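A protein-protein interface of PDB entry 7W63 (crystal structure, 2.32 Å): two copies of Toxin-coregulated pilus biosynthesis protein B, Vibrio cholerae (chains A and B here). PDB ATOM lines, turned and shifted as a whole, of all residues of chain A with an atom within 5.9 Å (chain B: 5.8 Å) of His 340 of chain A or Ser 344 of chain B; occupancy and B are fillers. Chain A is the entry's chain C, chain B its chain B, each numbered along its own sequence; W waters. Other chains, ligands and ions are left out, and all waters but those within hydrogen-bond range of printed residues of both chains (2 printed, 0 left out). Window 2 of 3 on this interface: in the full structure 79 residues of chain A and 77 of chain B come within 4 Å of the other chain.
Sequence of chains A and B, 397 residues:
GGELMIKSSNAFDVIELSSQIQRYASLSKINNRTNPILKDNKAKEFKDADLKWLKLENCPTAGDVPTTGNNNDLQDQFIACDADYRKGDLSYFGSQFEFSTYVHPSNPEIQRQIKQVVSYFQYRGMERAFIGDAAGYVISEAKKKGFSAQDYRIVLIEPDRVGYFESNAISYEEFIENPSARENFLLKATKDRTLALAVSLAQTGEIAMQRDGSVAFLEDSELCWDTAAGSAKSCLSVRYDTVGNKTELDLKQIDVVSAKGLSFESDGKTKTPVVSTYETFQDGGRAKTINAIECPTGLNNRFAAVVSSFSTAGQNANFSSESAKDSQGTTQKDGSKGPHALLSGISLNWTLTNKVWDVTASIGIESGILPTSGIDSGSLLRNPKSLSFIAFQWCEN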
ATOM      1  N   PHE A 310      31.518 -21.400  32.599  1.00  0.00           N
ATOM      2  CA  PHE A 310      30.720 -20.870  31.509  1.00  0.00           C
ATOM      3  C   PHE A 310      30.316 -21.948  30.527  1.00  0.00           C
ATOM      4  O   PHE A 310      31.016 -22.937  30.353  1.00  0.00           O
ATOM      5  CB  PHE A 310      31.489 -19.783  30.768  1.00  0.00           C
ATOM      6  CG  PHE A 310      32.734 -20.277  30.060  1.00  0.00           C
ATOM      7  CD1 PHE A 310      33.954 -20.309  30.716  1.00  0.00           C
ATOM      8  CD2 PHE A 310      32.688 -20.674  28.723  1.00  0.00           C
ATOM      9  CE1 PHE A 310      35.109 -20.725  30.058  1.00  0.00           C
ATOM     10  CE2 PHE A 310      33.830 -21.108  28.064  1.00  0.00           C
ATOM     11  CZ  PHE A 310      35.044 -21.133  28.732  1.00  0.00           C
ATOM     12  N   SER A 311      29.200 -21.747  29.852  1.00  0.00           N
ATOM     13  CA  SER A 311      28.930 -22.577  28.699  1.00  0.00           C
ATOM     14  C   SER A 311      28.140 -21.742  27.707  1.00  0.00           C
ATOM     15  O   SER A 311      27.814 -20.595  27.989  1.00  0.00           O
ATOM     16  CB  SER A 311      28.167 -23.849  29.091  1.00  0.00           C
ATOM     17  OG  SER A 311      26.790 -23.546  29.305  1.00  0.00           O
ATOM     18  N   THR A 312      27.830 -22.319  26.554  1.00  0.00           N
ATOM     19  CA  THR A 312      27.061 -21.622  25.534  1.00  0.00           C
ATOM     20  C   THR A 312      25.534 -21.846  25.661  1.00  0.00           C
ATOM     21  O   THR A 312      24.776 -21.608  24.714  1.00  0.00           O
ATOM     22  CB  THR A 312      27.539 -22.043  24.149  1.00  0.00           C
ATOM     23  OG1 THR A 312      27.472 -23.471  24.041  1.00  0.00           O
ATOM     24  CG2 THR A 312      29.015 -21.582  23.928  1.00  0.00           C
ATOM     25  N   ALA A 313      25.081 -22.274  26.842  1.00  0.00           N
ATOM     26  CA  ALA A 313      23.646 -22.532  27.065  1.00  0.00           C
ATOM     27  C   ALA A 313      22.819 -21.242  27.078  1.00  0.00           C
ATOM     28  O   ALA A 313      21.648 -21.242  26.690  1.00  0.00           O
ATOM     29  CB  ALA A 313      23.432 -23.317  28.370  1.00  0.00           C
ATOM     30  N   ASN A 316      19.500 -21.025  29.103  1.00  0.00           N
ATOM     31  CA  ASN A 316      19.084 -22.363  29.532  1.00  0.00           C
ATOM     32  C   ASN A 316      20.065 -22.972  30.510  1.00  0.00           C
ATOM     33  O   ASN A 316      20.719 -23.970  30.208  1.00  0.00           O
ATOM     34  CB  ASN A 316      18.919 -23.295  28.329  1.00  0.00           C
ATOM     35  CG  ASN A 316      18.208 -22.625  27.166  1.00  0.00           C
ATOM     36  OD1 ASN A 316      17.206 -21.922  27.352  1.00  0.00           O
ATOM     37  ND2 ASN A 316      18.735 -22.822  25.961  1.00  0.00           N
ATOM     38  N   SER A 327      23.226 -26.986  32.936  1.00  0.00           N
ATOM     39  CA  SER A 327      23.469 -26.435  31.604  1.00  0.00           C
ATOM     40  C   SER A 327      22.743 -27.273  30.567  1.00  0.00           C
ATOM     41  O   SER A 327      23.086 -28.439  30.369  1.00  0.00           O
ATOM     42  CB  SER A 327      24.972 -26.404  31.293  1.00  0.00           C
ATOM     43  OG  SER A 327      25.246 -25.583  30.174  1.00  0.00           O
ATOM     44  N   GLN A 328      21.756 -26.692  29.893  1.00  0.00           N
ATOM     45  CA  GLN A 328      20.873 -27.497  29.044  1.00  0.00           C
ATOM     46  C   GLN A 328      20.924 -27.206  27.545  1.00  0.00           C
ATOM     47  O   GLN A 328      19.930 -27.382  26.844  1.00  0.00           O
ATOM     48  CB  GLN A 328      19.447 -27.332  29.522  1.00  0.00           C
ATOM     49  CG  GLN A 328      19.234 -27.932  30.888  1.00  0.00           C
ATOM     50  CD  GLN A 328      17.869 -27.622  31.425  1.00  0.00           C
ATOM     51  OE1 GLN A 328      17.068 -28.527  31.661  1.00  0.00           O
ATOM     52  NE2 GLN A 328      17.582 -26.335  31.614  1.00  0.00           N
ATOM     53  N   GLY A 329      22.074 -26.754  27.057  1.00  0.00           N
ATOM     54  CA  GLY A 329      22.245 -26.530  25.639  1.00  0.00           C
ATOM     55  C   GLY A 329      21.728 -25.216  25.087  1.00  0.00           C
ATOM     56  O   GLY A 329      20.967 -24.477  25.726  1.00  0.00           O
ATOM     57  N   THR A 330      22.152 -24.936  23.862  1.00  0.00           N
ATOM     58  CA  THR A 330      21.832 -23.695  23.188  1.00  0.00           C
ATOM     59  C   THR A 330      20.458 -23.756  22.531  1.00  0.00           C
ATOM     60  O   THR A 330      20.068 -24.775  21.940  1.00  0.00           O
ATOM     61  CB  THR A 330      22.919 -23.365  22.135  1.00  0.00           C
ATOM     62  OG1 THR A 330      24.213 -23.571  22.722  1.00  0.00           O
ATOM     63  CG2 THR A 330      22.798 -21.928  21.644  1.00  0.00           C
ATOM     64  N   GLY A 338      18.924 -27.184  22.294  1.00  0.00           N
ATOM     65  CA  GLY A 338      19.658 -28.122  21.461  1.00  0.00           C
ATOM     66  C   GLY A 338      20.998 -28.476  22.059  1.00  0.00           C
ATOM     67  O   GLY A 338      21.199 -28.330  23.262  1.00  0.00           O
ATOM     68  N   PRO A 339      21.924 -28.963  21.232  1.00  0.00           N
ATOM     69  CA  PRO A 339      23.268 -29.195  21.777  1.00  0.00           C
ATOM     70  C   PRO A 339      23.961 -27.877  22.143  1.00  0.00           C
ATOM     71  O   PRO A 339      23.505 -26.789  21.769  1.00  0.00           O
ATOM     72  CB  PRO A 339      24.003 -29.913  20.631  1.00  0.00           C
ATOM     73  CG  PRO A 339      22.901 -30.430  19.718  1.00  0.00           C
ATOM     74  CD  PRO A 339      21.798 -29.411  19.836  1.00  0.00           C
ATOM     75  N   HIS A 340      25.049 -27.964  22.889  1.00  0.00           N
ATOM     76  CA  HIS A 340      25.801 -26.755  23.203  1.00  0.00           C
ATOM     77  C   HIS A 340      26.535 -26.272  21.951  1.00  0.00           C
ATOM     78  O   HIS A 340      27.257 -27.025  21.305  1.00  0.00           O
ATOM     79  CB  HIS A 340      26.760 -27.012  24.363  1.00  0.00           C
ATOM     80  CG  HIS A 340      26.068 -27.094  25.692  1.00  0.00           C
ATOM     81  ND1 HIS A 340      25.774 -28.292  26.311  1.00  0.00           N
ATOM     82  CD2 HIS A 340      25.573 -26.123  26.501  1.00  0.00           C
ATOM     83  CE1 HIS A 340      25.141 -28.056  27.446  1.00  0.00           C
ATOM     84  NE2 HIS A 340      25.006 -26.749  27.585  1.00  0.00           N
ATOM     85  N   ALA A 341      26.302 -25.020  21.586  1.00  0.00           N
ATOM     86  CA  ALA A 341      27.014 -24.416  20.472  1.00  0.00           C
ATOM     87  C   ALA A 341      28.496 -24.225  20.831  1.00  0.00           C
ATOM     88  O   ALA A 341      28.872 -24.246  22.009  1.00  0.00           O
ATOM     89  CB  ALA A 341      26.373 -23.078  20.089  1.00  0.00           C
ATOM     90  N   LEU A 342      29.320 -24.039  19.805  1.00  0.00           N
ATOM     91  CA  LEU A 342      30.736 -23.727  19.977  1.00  0.00           C
ATOM     92  C   LEU A 342      30.961 -22.225  20.218  1.00  0.00           C
ATOM     93  O   LEU A 342      30.208 -21.374  19.735  1.00  0.00           O
ATOM     94  CB  LEU A 342      31.524 -24.215  18.756  1.00  0.00           C
ATOM     95  CG  LEU A 342      31.438 -25.739  18.537  1.00  0.00           C
ATOM     96  CD1 LEU A 342      32.068 -26.181  17.210  1.00  0.00           C
ATOM     97  CD2 LEU A 342      32.078 -26.483  19.705  1.00  0.00           C
ATOM     98  N   LEU A 343      32.023 -21.914  20.953  1.00  0.00           N
ATOM     99  CA  LEU A 343      32.257 -20.565  21.487  1.00  0.00           C
ATOM    100  C   LEU A 343      33.356 -19.761  20.752  1.00  0.00           C
ATOM    101  O   LEU A 343      34.366 -20.333  20.333  1.00  0.00           O
ATOM    102  CB  LEU A 343      32.613 -20.706  22.963  1.00  0.00           C
ATOM    103  CG  LEU A 343      32.896 -19.486  23.815  1.00  0.00           C
ATOM    104  CD1 LEU A 343      32.085 -19.610  25.089  1.00  0.00           C
ATOM    105  CD2 LEU A 343      34.359 -19.489  24.140  1.00  0.00           C
ATOM    106  N   GLU A 366      29.294 -19.561  17.567  1.00  0.00           N
ATOM    107  CA  GLU A 366      29.200 -19.809  16.132  1.00  0.00           C
ATOM    108  C   GLU A 366      27.852 -19.351  15.586  1.00  0.00           C
ATOM    109  O   GLU A 366      26.855 -19.298  16.322  1.00  0.00           O
ATOM    110  CB  GLU A 366      29.411 -21.294  15.816  1.00  0.00           C
ATOM    111  CG  GLU A 366      28.519 -22.220  16.612  1.00  0.00           C
ATOM    112  CD  GLU A 366      28.577 -23.656  16.128  1.00  0.00           C
ATOM    113  OE1 GLU A 366      28.786 -23.872  14.912  1.00  0.00           O
ATOM    114  OE2 GLU A 366      28.411 -24.569  16.967  1.00  0.00           O
ATOM    115  N   LEU B 342      37.204 -28.236  19.295  1.00  0.00           N
ATOM    116  CA  LEU B 342      36.660 -26.931  19.637  1.00  0.00           C
ATOM    117  C   LEU B 342      35.817 -27.020  20.921  1.00  0.00           C
ATOM    118  O   LEU B 342      35.270 -28.073  21.242  1.00  0.00           O
ATOM    119  CB  LEU B 342      35.833 -26.382  18.462  1.00  0.00           C
ATOM    120  CG  LEU B 342      36.675 -26.237  17.183  1.00  0.00           C
ATOM    121  CD1 LEU B 342      35.820 -25.908  15.952  1.00  0.00           C
ATOM    122  CD2 LEU B 342      37.744 -25.178  17.390  1.00  0.00           C
ATOM    123  N   LEU B 343      35.693 -25.898  21.628  1.00  0.00           N
ATOM    124  CA  LEU B 343      35.194 -25.875  23.004  1.00  0.00           C
ATOM    125  C   LEU B 343      33.799 -25.255  23.118  1.00  0.00           C
ATOM    126  O   LEU B 343      33.492 -24.305  22.403  1.00  0.00           O
ATOM    127  CB  LEU B 343      36.192 -25.100  23.869  1.00  0.00           C
ATOM    128  CG  LEU B 343      35.981 -24.965  25.368  1.00  0.00           C
ATOM    129  CD1 LEU B 343      37.311 -25.128  26.051  1.00  0.00           C
ATOM    130  CD2 LEU B 343      35.387 -23.608  25.694  1.00  0.00           C
ATOM    131  N   SER B 344      32.961 -25.783  24.016  1.00  0.00           N
ATOM    132  CA  SER B 344      31.642 -25.184  24.277  1.00  0.00           C
ATOM    133  C   SER B 344      31.485 -24.634  25.703  1.00  0.00           C
ATOM    134  O   SER B 344      30.552 -23.891  25.983  1.00  0.00           O
ATOM    135  CB  SER B 344      30.519 -26.199  24.034  1.00  0.00           C
ATOM    136  OG  SER B 344      30.715 -27.359  24.837  1.00  0.00           O
ATOM    137  N   GLY B 345      32.370 -25.023  26.615  1.00  0.00           N
ATOM    138  CA  GLY B 345      32.240 -24.577  27.985  1.00  0.00           C
ATOM    139  C   GLY B 345      33.235 -25.161  28.959  1.00  0.00           C
ATOM    140  O   GLY B 345      33.959 -26.102  28.629  1.00  0.00           O
ATOM    141  N   ILE B 346      33.293 -24.565  30.151  1.00  0.00           N
ATOM    142  CA  ILE B 346      34.096 -25.071  31.262  1.00  0.00           C
ATOM    143  C   ILE B 346      33.275 -24.973  32.550  1.00  0.00           C
ATOM    144  O   ILE B 346      32.646 -23.946  32.815  1.00  0.00           O
ATOM    145  CB  ILE B 346      35.412 -24.305  31.429  1.00  0.00           C
ATOM    146  CG1 ILE B 346      36.237 -24.329  30.136  1.00  0.00           C
ATOM    147  CG2 ILE B 346      36.211 -24.884  32.614  1.00  0.00           C
ATOM    148  CD1 ILE B 346      37.560 -23.557  30.232  1.00  0.00           C
ATOM    149  N   GLY B 364      33.482 -28.968  28.147  1.00  0.00           N
ATOM    150  CA  GLY B 364      32.612 -29.399  27.065  1.00  0.00           C
ATOM    151  C   GLY B 364      33.180 -29.098  25.682  1.00  0.00           C
ATOM    152  O   GLY B 364      33.604 -27.963  25.410  1.00  0.00           O
ATOM    153  N   ILE B 365      33.215 -30.106  24.810  1.00  0.00           N
ATOM    154  CA  ILE B 365      33.730 -29.922  23.443  1.00  0.00           C
ATOM    155  C   ILE B 365      32.712 -30.336  22.379  1.00  0.00           C
ATOM    156  O   ILE B 365      31.617 -30.807  22.700  1.00  0.00           O
ATOM    157  CB  ILE B 365      35.052 -30.696  23.228  1.00  0.00           C
ATOM    158  CG1 ILE B 365      34.804 -32.207  23.187  1.00  0.00           C
ATOM    159  CG2 ILE B 365      36.067 -30.342  24.303  1.00  0.00           C
ATOM    160  CD1 ILE B 365      36.013 -32.993  22.760  1.00  0.00           C
ATOM    161  N   GLU B 366      33.077 -30.151  21.110  1.00  0.00           N
ATOM    162  CA  GLU B 366      32.211 -30.541  19.998  1.00  0.00           C
ATOM    163  C   GLU B 366      31.999 -32.051  20.005  1.00  0.00           C
ATOM    164  O   GLU B 366      32.882 -32.819  20.402  1.00  0.00           O
ATOM    165  CB  GLU B 366      32.799 -30.099  18.657  1.00  0.00           C
ATOM    166  CG  GLU B 366      34.267 -30.484  18.466  1.00  0.00           C
ATOM    167  CD  GLU B 366      34.832 -29.998  17.128  1.00  0.00           C
ATOM    168  OE1 GLU B 366      34.056 -29.907  16.147  1.00  0.00           O
ATOM    169  OE2 GLU B 366      36.051 -29.699  17.063  1.00  0.00           O
ATOM    170  N   SER B 379      31.104 -35.924  25.077  1.00  0.00           N
ATOM    171  CA  SER B 379      31.319 -34.537  24.687  1.00  0.00           C
ATOM    172  C   SER B 379      32.016 -33.791  25.809  1.00  0.00           C
ATOM    173  O   SER B 379      31.968 -32.562  25.862  1.00  0.00           O
ATOM    174  CB  SER B 379      29.988 -33.856  24.361  1.00  0.00           C
ATOM    175  OG  SER B 379      29.552 -34.178  23.054  1.00  0.00           O
HETATM  176  O   HOH W   1      29.995 -25.333  31.597  1.00  0.00           O
HETATM  177  O   HOH W   2      34.647 -22.981  20.022  1.00  0.00           O
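The backbone carbonyl oxygen (O) of Leu 343 of chain B lies within hydrogen-bond range of the backbone NH (N) of Leu 343 of chain A, at 3.2 Å.
The backbone NH (N) of Thr 312 of chain A sits at hydrogen-bond distance from the backbone carbonyl oxygen (O) of Ser 344 of chain B.
The backbone NH (N) of Phe 310 of chain A lies within hydrogen-bond range of the backbone carbonyl oxygen (O) of Ile 346 of chain B, at 2.8 Å.
N of Leu 342 of chain B sits at hydrogen-bond distance from OE2 of Glu 366 of chain B.
The backbone NH (N) of Ser 344 of chain B is in hydrogen-bond range of the backbone carbonyl oxygen (O) of Gly 364 of chain B, 2.7 Å away.
OG of Ser 311 of chain A lies close to N of Ala 313 of chain A (3.3 Å).
The side-chain hydroxyl of Ser 327 of chain A sits at hydrogen-bond distance from the side-chain hydroxyl of Ser 311 of chain A.
A ring nitrogen (NE2) of His 340 of chain A is in hydrogen-bond range of the backbone NH (N) of Gly 329 of chain A (3.0 Å).
OG1 of Thr 330 of chain A is in hydrogen-bond range of N of Ala 341 of chain A (2.8 Å).
Among the printed residues, merely in contact across the chains: Phe 310 of chain A with Gly 345 of chain B (3.1 Å), Ala 341 of chain A with Ser 344 of chain B (3.3 Å), Ser 311 of chain A with Ser 344 of chain B (3.4 Å), Leu 342 of chain A with Leu 343 of chain B (3.7 Å), Phe 310 of chain A with Leu 343 of chain B (3.8 Å), Leu 342 of chain A with Glu 366 of chain B (3.8 Å), His 340 of chain A with Ser 344 of chain B (3.9 Å), Leu 342 of chain A with Leu 342 of chain B (3.9 Å) and Ser 311 of chain A with Gly 345 of chain B (3.9 Å).
Ser 344 of chain B touches four residues of chain A.
Of the printed residues of chain B, Leu 343 of chain A touches Leu 343.
Printed residues of chain A within 4 Å of Leu 343 of chain B: Phe 310 (3.8 Å), Leu 342 (3.7 Å) and Leu 343 (3.2 Å).
Of the printed residues of chain B, Phe 310 of chain A touches Leu 343, Gly 345 and Ile 346.
Asn 316 of chain A touches none of the printed residues of chain B.
Ser 327 of chain A touches none of the printed residues of chain B.
The nearest printed residue of chain B that does not touch His 340 of chain A is Ile 365 of chain B (5.9 Å).
Among the printed residues, 12 pairs touch across the chains.
Among the printed residues, no Asp or Glu carboxylate lies within 4 Å of a Lys or Arg side-chain nitrogen of the other chain.
Leu 342 of chain A touches its own counterpart, Leu 342 of chain B.
Leu 342 of chain A touches Leu 343 of chain B, but with the chains exchanged Leu 343 of chain A does not touch Leu 342 of chain B (6.4 Å).
Leu 342 of chain A touches Glu 366 of chain B, but with the chains exchanged Glu 366 of chain A does not touch Leu 342 of chain B (7.4 Å).
Leu 343 of chain A touches its own counterpart, Leu 343 of chain B.
Positions printed for both chains: 342, 343 and 366.
Water W2 bridges the backbone carbonyl oxygen (O) of Leu 343 of chain A (2.7 Å) and the backbone carbonyl oxygen (O) of Leu 343 of chain B (3.0 Å).
Water W1 bridges the backbone carbonyl oxygen (O) of Phe 310 of chain A and the backbone carbonyl oxygen (O) of Ile 346 of chain B.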
